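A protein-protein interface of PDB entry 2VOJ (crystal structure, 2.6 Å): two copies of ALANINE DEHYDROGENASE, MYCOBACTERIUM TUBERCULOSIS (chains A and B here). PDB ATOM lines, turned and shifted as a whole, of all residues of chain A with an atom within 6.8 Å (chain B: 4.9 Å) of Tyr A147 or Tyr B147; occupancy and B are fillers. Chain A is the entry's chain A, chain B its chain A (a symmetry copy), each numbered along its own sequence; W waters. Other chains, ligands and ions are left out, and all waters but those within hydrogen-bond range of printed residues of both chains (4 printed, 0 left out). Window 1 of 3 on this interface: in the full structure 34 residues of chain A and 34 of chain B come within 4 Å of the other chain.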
ATOM      1  N   ALA A 142     -17.597   6.713  22.996  1.00  0.00           N
ATOM      2  CA  ALA A 142     -17.462   7.354  21.696  1.00  0.00           C
ATOM      3  C   ALA A 142     -17.729   8.837  21.798  1.00  0.00           C
ATOM      4  O   ALA A 142     -17.009   9.613  21.201  1.00  0.00           O
ATOM      5  CB  ALA A 142     -18.399   6.728  20.670  1.00  0.00           C
ATOM      6  N   GLN A 143     -18.795   9.215  22.519  1.00  0.00           N
ATOM      7  CA  GLN A 143     -19.107  10.617  22.839  1.00  0.00           C
ATOM      8  C   GLN A 143     -17.940  11.363  23.489  1.00  0.00           C
ATOM      9  O   GLN A 143     -17.511  12.364  22.973  1.00  0.00           O
ATOM     10  CB  GLN A 143     -20.298  10.701  23.803  1.00  0.00           C
ATOM     11  CG  GLN A 143     -21.581  10.978  23.145  1.00  0.00           C
ATOM     12  CD  GLN A 143     -22.784  10.526  23.957  1.00  0.00           C
ATOM     13  OE1 GLN A 143     -23.056  11.093  25.029  1.00  0.00           O
ATOM     14  NE2 GLN A 143     -23.509   9.469  23.446  1.00  0.00           N
ATOM     15  N   VAL A 144     -17.452  10.861  24.622  1.00  0.00           N
ATOM     16  CA  VAL A 144     -16.430  11.536  25.386  1.00  0.00           C
ATOM     17  C   VAL A 144     -15.099  11.502  24.638  1.00  0.00           C
ATOM     18  O   VAL A 144     -14.368  12.499  24.632  1.00  0.00           O
ATOM     19  CB  VAL A 144     -16.334  11.046  26.899  1.00  0.00           C
ATOM     20  CG1 VAL A 144     -17.706  11.135  27.593  1.00  0.00           C
ATOM     21  CG2 VAL A 144     -15.756   9.617  27.044  1.00  0.00           C
ATOM     22  N   GLY A 145     -14.813  10.389  23.965  1.00  0.00           N
ATOM     23  CA  GLY A 145     -13.673  10.334  23.045  1.00  0.00           C
ATOM     24  C   GLY A 145     -13.717  11.396  21.962  1.00  0.00           C
ATOM     25  O   GLY A 145     -12.725  12.050  21.709  1.00  0.00           O
ATOM     26  N   ALA A 146     -14.874  11.570  21.331  1.00  0.00           N
ATOM     27  CA  ALA A 146     -15.071  12.597  20.314  1.00  0.00           C
ATOM     28  C   ALA A 146     -14.728  13.994  20.872  1.00  0.00           C
ATOM     29  O   ALA A 146     -14.013  14.790  20.235  1.00  0.00           O
ATOM     30  CB  ALA A 146     -16.494  12.566  19.832  1.00  0.00           C
ATOM     31  N   TYR A 147     -15.243  14.260  22.075  1.00  0.00           N
ATOM     32  CA  TYR A 147     -15.089  15.520  22.730  1.00  0.00           C
ATOM     33  C   TYR A 147     -13.611  15.855  23.032  1.00  0.00           C
ATOM     34  O   TYR A 147     -13.128  16.944  22.726  1.00  0.00           O
ATOM     35  CB  TYR A 147     -15.921  15.496  24.006  1.00  0.00           C
ATOM     36  CG  TYR A 147     -16.156  16.874  24.547  1.00  0.00           C
ATOM     37  CD1 TYR A 147     -17.147  17.677  24.007  1.00  0.00           C
ATOM     38  CD2 TYR A 147     -15.367  17.395  25.569  1.00  0.00           C
ATOM     39  CE1 TYR A 147     -17.367  18.939  24.486  1.00  0.00           C
ATOM     40  CE2 TYR A 147     -15.575  18.679  26.063  1.00  0.00           C
ATOM     41  CZ  TYR A 147     -16.573  19.438  25.510  1.00  0.00           C
ATOM     42  OH  TYR A 147     -16.823  20.709  25.951  1.00  0.00           O
ATOM     43  N   HIS A 148     -12.894  14.900  23.627  1.00  0.00           N
ATOM     44  CA  HIS A 148     -11.493  15.104  24.026  1.00  0.00           C
ATOM     45  C   HIS A 148     -10.525  15.065  22.854  1.00  0.00           C
ATOM     46  O   HIS A 148      -9.341  15.293  23.027  1.00  0.00           O
ATOM     47  CB  HIS A 148     -11.072  14.124  25.123  1.00  0.00           C
ATOM     48  CG  HIS A 148     -11.838  14.322  26.391  1.00  0.00           C
ATOM     49  ND1 HIS A 148     -11.412  15.173  27.390  1.00  0.00           N
ATOM     50  CD2 HIS A 148     -13.050  13.863  26.780  1.00  0.00           C
ATOM     51  CE1 HIS A 148     -12.309  15.202  28.358  1.00  0.00           C
ATOM     52  NE2 HIS A 148     -13.318  14.425  28.010  1.00  0.00           N
ATOM     53  N   LEU A 149     -11.030  14.809  21.655  1.00  0.00           N
ATOM     54  CA  LEU A 149     -10.208  14.922  20.470  1.00  0.00           C
ATOM     55  C   LEU A 149     -10.068  16.390  20.010  1.00  0.00           C
ATOM     56  O   LEU A 149      -9.209  16.703  19.196  1.00  0.00           O
ATOM     57  CB  LEU A 149     -10.787  14.028  19.366  1.00  0.00           C
ATOM     58  CG  LEU A 149      -9.931  12.995  18.655  1.00  0.00           C
ATOM     59  CD1 LEU A 149      -8.701  12.600  19.415  1.00  0.00           C
ATOM     60  CD2 LEU A 149     -10.761  11.792  18.333  1.00  0.00           C
ATOM     61  N   MET A 150     -10.907  17.278  20.537  1.00  0.00           N
ATOM     62  CA  MET A 150     -10.781  18.724  20.261  1.00  0.00           C
ATOM     63  C   MET A 150      -9.497  19.304  20.874  1.00  0.00           C
ATOM     64  O   MET A 150      -9.137  18.953  22.000  1.00  0.00           O
ATOM     65  CB  MET A 150     -12.000  19.488  20.786  1.00  0.00           C
ATOM     66  CG  MET A 150     -13.328  18.919  20.386  1.00  0.00           C
ATOM     67  SD  MET A 150     -14.702  20.012  20.686  1.00  0.00           S
ATOM     68  CE  MET A 150     -14.685  20.117  22.446  1.00  0.00           C
ATOM     69  N   ARG A 151      -8.820  20.194  20.147  1.00  0.00           N
ATOM     70  CA  ARG A 151      -7.538  20.756  20.628  1.00  0.00           C
ATOM     71  C   ARG A 151      -7.736  21.506  21.940  1.00  0.00           C
ATOM     72  O   ARG A 151      -6.915  21.486  22.828  1.00  0.00           O
ATOM     73  CB  ARG A 151      -6.829  21.638  19.583  1.00  0.00           C
ATOM     74  CG  ARG A 151      -5.305  21.454  19.645  1.00  0.00           C
ATOM     75  CD  ARG A 151      -4.545  22.725  19.336  1.00  0.00           C
ATOM     76  NE  ARG A 151      -3.303  22.795  20.099  1.00  0.00           N
ATOM     77  CZ  ARG A 151      -3.196  23.252  21.356  1.00  0.00           C
ATOM     78  NH1 ARG A 151      -4.259  23.705  22.023  1.00  0.00           N
ATOM     79  NH2 ARG A 151      -2.015  23.253  21.963  1.00  0.00           N
ATOM     80  N   THR A 152      -8.886  22.133  22.020  1.00  0.00           N
ATOM     81  CA  THR A 152      -9.389  22.781  23.187  1.00  0.00           C
ATOM     82  C   THR A 152      -9.405  21.929  24.489  1.00  0.00           C
ATOM     83  O   THR A 152      -9.447  22.460  25.595  1.00  0.00           O
ATOM     84  CB  THR A 152     -10.745  23.290  22.794  1.00  0.00           C
ATOM     85  OG1 THR A 152     -10.639  24.704  22.640  1.00  0.00           O
ATOM     86  CG2 THR A 152     -11.807  22.923  23.775  1.00  0.00           C
ATOM     87  N   GLN A 153      -9.374  20.609  24.366  1.00  0.00           N
ATOM     88  CA  GLN A 153      -9.332  19.745  25.553  1.00  0.00           C
ATOM     89  C   GLN A 153      -8.028  18.980  25.629  1.00  0.00           C
ATOM     90  O   GLN A 153      -7.936  18.038  26.397  1.00  0.00           O
ATOM     91  CB  GLN A 153     -10.480  18.718  25.601  1.00  0.00           C
ATOM     92  CG  GLN A 153     -11.854  19.269  25.299  1.00  0.00           C
ATOM     93  CD  GLN A 153     -12.399  20.061  26.431  1.00  0.00           C
ATOM     94  OE1 GLN A 153     -12.350  19.627  27.572  1.00  0.00           O
ATOM     95  NE2 GLN A 153     -12.908  21.247  26.134  1.00  0.00           N
ATOM     96  N   GLY A 155      -6.644  17.238  22.978  1.00  0.00           N
ATOM     97  CA  GLY A 155      -6.523  16.261  21.877  1.00  0.00           C
ATOM     98  C   GLY A 155      -5.880  16.803  20.607  1.00  0.00           C
ATOM     99  O   GLY A 155      -5.548  17.985  20.531  1.00  0.00           O
ATOM    100  N   MET A 160     -14.309  13.819  14.565  1.00  0.00           N
ATOM    101  CA  MET A 160     -14.632  12.386  14.412  1.00  0.00           C
ATOM    102  C   MET A 160     -14.867  11.979  12.973  1.00  0.00           C
ATOM    103  O   MET A 160     -14.196  11.080  12.493  1.00  0.00           O
ATOM    104  CB  MET A 160     -15.886  12.004  15.209  1.00  0.00           C
ATOM    105  CG  MET A 160     -15.630  11.673  16.642  1.00  0.00           C
ATOM    106  SD  MET A 160     -14.630  10.215  16.878  1.00  0.00           S
ATOM    107  CE  MET A 160     -15.784   8.931  17.366  1.00  0.00           C
ATOM    108  N   VAL A 263      -6.357  10.033  22.045  1.00  0.00           N
ATOM    109  CA  VAL A 263      -7.057   9.757  23.278  1.00  0.00           C
ATOM    110  C   VAL A 263      -7.368   8.297  23.468  1.00  0.00           C
ATOM    111  O   VAL A 263      -7.697   7.596  22.515  1.00  0.00           O
ATOM    112  CB  VAL A 263      -8.229  10.762  23.644  1.00  0.00           C
ATOM    113  CG1 VAL A 263      -8.453  11.797  22.623  1.00  0.00           C
ATOM    114  CG2 VAL A 263      -9.494  10.072  24.044  1.00  0.00           C
ATOM    115  N   TYR A 283     -15.189  11.749  37.522  1.00  0.00           N
ATOM    116  CA  TYR A 283     -15.788  12.816  36.716  1.00  0.00           C
ATOM    117  C   TYR A 283     -15.309  14.236  37.031  1.00  0.00           C
ATOM    118  O   TYR A 283     -15.450  15.113  36.182  1.00  0.00           O
ATOM    119  CB  TYR A 283     -17.321  12.756  36.740  1.00  0.00           C
ATOM    120  CG  TYR A 283     -17.903  11.891  35.649  1.00  0.00           C
ATOM    121  CD1 TYR A 283     -18.671  10.764  35.967  1.00  0.00           C
ATOM    122  CD2 TYR A 283     -17.685  12.186  34.290  1.00  0.00           C
ATOM    123  CE1 TYR A 283     -19.200   9.946  34.978  1.00  0.00           C
ATOM    124  CE2 TYR A 283     -18.204  11.372  33.285  1.00  0.00           C
ATOM    125  CZ  TYR A 283     -18.970  10.249  33.640  1.00  0.00           C
ATOM    126  OH  TYR A 283     -19.510   9.425  32.670  1.00  0.00           O
ATOM    127  N   PRO A 286     -11.274  13.649  35.101  1.00  0.00           N
ATOM    128  CA  PRO A 286     -11.388  12.450  34.288  1.00  0.00           C
ATOM    129  C   PRO A 286     -10.125  12.020  33.531  1.00  0.00           C
ATOM    130  O   PRO A 286      -9.964  10.835  33.246  1.00  0.00           O
ATOM    131  CB  PRO A 286     -12.497  12.813  33.302  1.00  0.00           C
ATOM    132  CG  PRO A 286     -12.432  14.284  33.182  1.00  0.00           C
ATOM    133  CD  PRO A 286     -12.042  14.778  34.530  1.00  0.00           C
ATOM    134  N   TYR A 296      -8.405   8.577  29.463  1.00  0.00           N
ATOM    135  CA  TYR A 296      -9.675   8.838  30.098  1.00  0.00           C
ATOM    136  C   TYR A 296     -10.060   7.523  30.775  1.00  0.00           C
ATOM    137  O   TYR A 296     -10.155   6.469  30.113  1.00  0.00           O
ATOM    138  CB  TYR A 296     -10.694   9.290  29.034  1.00  0.00           C
ATOM    139  CG  TYR A 296     -12.041   9.710  29.546  1.00  0.00           C
ATOM    140  CD1 TYR A 296     -12.442  11.048  29.504  1.00  0.00           C
ATOM    141  CD2 TYR A 296     -12.941   8.769  30.054  1.00  0.00           C
ATOM    142  CE1 TYR A 296     -13.689  11.440  29.991  1.00  0.00           C
ATOM    143  CE2 TYR A 296     -14.184   9.145  30.541  1.00  0.00           C
ATOM    144  CZ  TYR A 296     -14.546  10.467  30.502  1.00  0.00           C
ATOM    145  OH  TYR A 296     -15.779  10.811  30.970  1.00  0.00           O
ATOM    146  N   GLN B 143     -21.919  16.621  18.696  1.00  0.00           N
ATOM    147  CA  GLN B 143     -20.903  16.181  19.666  1.00  0.00           C
ATOM    148  C   GLN B 143     -20.983  16.920  21.003  1.00  0.00           C
ATOM    149  O   GLN B 143     -21.138  16.293  22.021  1.00  0.00           O
ATOM    150  CB  GLN B 143     -19.490  16.400  19.107  1.00  0.00           C
ATOM    151  CG  GLN B 143     -18.886  15.195  18.523  1.00  0.00           C
ATOM    152  CD  GLN B 143     -17.790  15.501  17.515  1.00  0.00           C
ATOM    153  OE1 GLN B 143     -16.725  16.017  17.893  1.00  0.00           O
ATOM    154  NE2 GLN B 143     -18.064  15.192  16.197  1.00  0.00           N
ATOM    155  N   VAL B 144     -20.868  18.246  20.975  1.00  0.00           N
ATOM    156  CA  VAL B 144     -20.815  19.041  22.179  1.00  0.00           C
ATOM    157  C   VAL B 144     -22.172  19.038  22.877  1.00  0.00           C
ATOM    158  O   VAL B 144     -22.233  18.956  24.109  1.00  0.00           O
ATOM    159  CB  VAL B 144     -20.204  20.496  21.958  1.00  0.00           C
ATOM    160  CG1 VAL B 144     -18.826  20.415  21.276  1.00  0.00           C
ATOM    161  CG2 VAL B 144     -21.140  21.437  21.160  1.00  0.00           C
ATOM    162  N   GLY B 145     -23.253  19.066  22.098  1.00  0.00           N
ATOM    163  CA  GLY B 145     -24.591  18.849  22.653  1.00  0.00           C
ATOM    164  C   GLY B 145     -24.732  17.534  23.398  1.00  0.00           C
ATOM    165  O   GLY B 145     -25.267  17.505  24.488  1.00  0.00           O
ATOM    166  N   ALA B 146     -24.243  16.448  22.807  1.00  0.00           N
ATOM    167  CA  ALA B 146     -24.256  15.133  23.439  1.00  0.00           C
ATOM    168  C   ALA B 146     -23.547  15.175  24.808  1.00  0.00           C
ATOM    169  O   ALA B 146     -24.057  14.659  25.820  1.00  0.00           O
ATOM    170  CB  ALA B 146     -23.588  14.133  22.539  1.00  0.00           C
ATOM    171  N   TYR B 147     -22.371  15.811  24.813  1.00  0.00           N
ATOM    172  CA  TYR B 147     -21.537  15.902  25.968  1.00  0.00           C
ATOM    173  C   TYR B 147     -22.214  16.661  27.131  1.00  0.00           C
ATOM    174  O   TYR B 147     -22.243  16.192  28.267  1.00  0.00           O
ATOM    175  CB  TYR B 147     -20.231  16.573  25.557  1.00  0.00           C
ATOM    176  CG  TYR B 147     -19.148  16.354  26.570  1.00  0.00           C
ATOM    177  CD1 TYR B 147     -18.441  15.164  26.590  1.00  0.00           C
ATOM    178  CD2 TYR B 147     -18.852  17.316  27.533  1.00  0.00           C
ATOM    179  CE1 TYR B 147     -17.454  14.949  27.513  1.00  0.00           C
ATOM    180  CE2 TYR B 147     -17.856  17.110  28.482  1.00  0.00           C
ATOM    181  CZ  TYR B 147     -17.171  15.923  28.462  1.00  0.00           C
ATOM    182  OH  TYR B 147     -16.183  15.660  29.371  1.00  0.00           O
ATOM    183  N   HIS B 148     -22.770  17.836  26.831  1.00  0.00           N
ATOM    184  CA  HIS B 148     -23.396  18.692  27.850  1.00  0.00           C
ATOM    185  C   HIS B 148     -24.759  18.190  28.298  1.00  0.00           C
ATOM    186  O   HIS B 148     -25.360  18.759  29.193  1.00  0.00           O
ATOM    187  CB  HIS B 148     -23.465  20.151  27.395  1.00  0.00           C
ATOM    188  CG  HIS B 148     -22.113  20.755  27.202  1.00  0.00           C
ATOM    189  ND1 HIS B 148     -21.439  21.407  28.215  1.00  0.00           N
ATOM    190  CD2 HIS B 148     -21.263  20.719  26.149  1.00  0.00           C
ATOM    191  CE1 HIS B 148     -20.248  21.780  27.785  1.00  0.00           C
ATOM    192  NE2 HIS B 148     -20.110  21.366  26.538  1.00  0.00           N
ATOM    193  N   LEU B 149     -25.235  17.106  27.702  1.00  0.00           N
ATOM    194  CA  LEU B 149     -26.441  16.468  28.185  1.00  0.00           C
ATOM    195  C   LEU B 149     -26.161  15.574  29.413  1.00  0.00           C
ATOM    196  O   LEU B 149     -27.086  15.172  30.108  1.00  0.00           O
ATOM    197  CB  LEU B 149     -27.091  15.683  27.039  1.00  0.00           C
ATOM    198  CG  LEU B 149     -28.544  15.899  26.657  1.00  0.00           C
ATOM    199  CD1 LEU B 149     -29.105  17.209  27.122  1.00  0.00           C
ATOM    200  CD2 LEU B 149     -28.700  15.756  25.175  1.00  0.00           C
ATOM    201  N   MET B 150     -24.892  15.274  29.674  1.00  0.00           N
ATOM    202  CA  MET B 150     -24.503  14.531  30.891  1.00  0.00           C
ATOM    203  C   MET B 150     -24.759  15.356  32.161  1.00  0.00           C
ATOM    204  O   MET B 150     -24.494  16.560  32.178  1.00  0.00           O
ATOM    205  CB  MET B 150     -23.031  14.112  30.828  1.00  0.00           C
ATOM    206  CG  MET B 150     -22.617  13.433  29.557  1.00  0.00           C
ATOM    207  SD  MET B 150     -21.028  12.634  29.651  1.00  0.00           S
ATOM    208  CE  MET B 150     -19.957  14.015  29.882  1.00  0.00           C
ATOM    209  N   GLN B 153     -22.212  17.699  33.554  1.00  0.00           N
ATOM    210  CA  GLN B 153     -21.922  19.017  32.975  1.00  0.00           C
ATOM    211  C   GLN B 153     -23.098  19.958  33.134  1.00  0.00           C
ATOM    212  O   GLN B 153     -23.122  20.992  32.490  1.00  0.00           O
ATOM    213  CB  GLN B 153     -21.567  18.962  31.477  1.00  0.00           C
ATOM    214  CG  GLN B 153     -20.571  17.894  31.088  1.00  0.00           C
ATOM    215  CD  GLN B 153     -19.186  18.249  31.492  1.00  0.00           C
ATOM    216  OE1 GLN B 153     -18.738  19.362  31.260  1.00  0.00           O
ATOM    217  NE2 GLN B 153     -18.494  17.313  32.123  1.00  0.00           N
HETATM  218  O   HOH W   1     -25.672  12.179  26.222  1.00  0.00           O
HETATM  219  O   HOH W   2     -17.043  15.409  33.256  1.00  0.00           O
HETATM  220  O   HOH W   3     -13.771  15.393  17.319  1.00  0.00           O
HETATM  221  O   HOH W   4     -15.964  13.473  31.102  1.00  0.00           O
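Water W2 lies within hydrogen-bond range of the side-chain amide nitrogen of Gln B153 (2.6 Å) and the backbone carbonyl oxygen of Tyr A283 (3.3 Å). Water W4 bridges the side-chain hydroxyl (OH) of Tyr A296 (2.7 Å) and the side-chain hydroxyl (OH) of Tyr B147 (2.8 Å). Water W3 lies within hydrogen-bond range of the backbone carbonyl oxygen (O) of Ala A146, the side-chain amide oxygen (OE1) of Gln B143 and the backbone NH (N) of Met A160. Water W1 bridges O of Ala B146 and OE1 of Gln A143.
Gln A143 touches Ala B146, and with the chains exchanged Ala A146 touches Gln B143. Val A144 touches Tyr B147, and with the chains exchanged Tyr A147 touches Val B144. Tyr B147 touches its own counterpart, Tyr A147. Tyr A147 touches His B148, and with the chains exchanged His A148 touches Tyr B147. 9 positions are printed for both chains.
Among the printed residues, merely in contact across the chains: Tyr A147 with Tyr B147, Gln A143 with Ala B146, Ala A146 with Gln B143, Tyr A147 with Val B144, Val A144 with Tyr B147 and Met A160 with Gln B143.
NE2 of His B148 is in hydrogen-bond range of OH of Tyr A147. A ring nitrogen (NE2) of His A148 sits at hydrogen-bond distance from the side-chain hydroxyl (OH) of Tyr B147 (3.4 Å).
O of His A148 lies close to N of Gly A155, 3.3 Å away.
Of the 18 printed residues of chain A, 6 touch a printed residue of chain B. Hydrophobic or aromatic side chains of chain B that line the printed part of chain A: Val B144, Ala B146, Tyr B147 and His B148.
Tyr A147 touches just these residues of chain B: Val B144, Tyr B147 and His B148. Tyr B147 touches just these residues of chain A: Val A144, Tyr A147 and His A148. Printed residues of chain A within 4 Å of Val B144: Tyr A147. Printed residues of chain A within 4 Å of Gln B143: Ala A146 and Met A160. Val A263 touches none of the printed residues of chain B.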
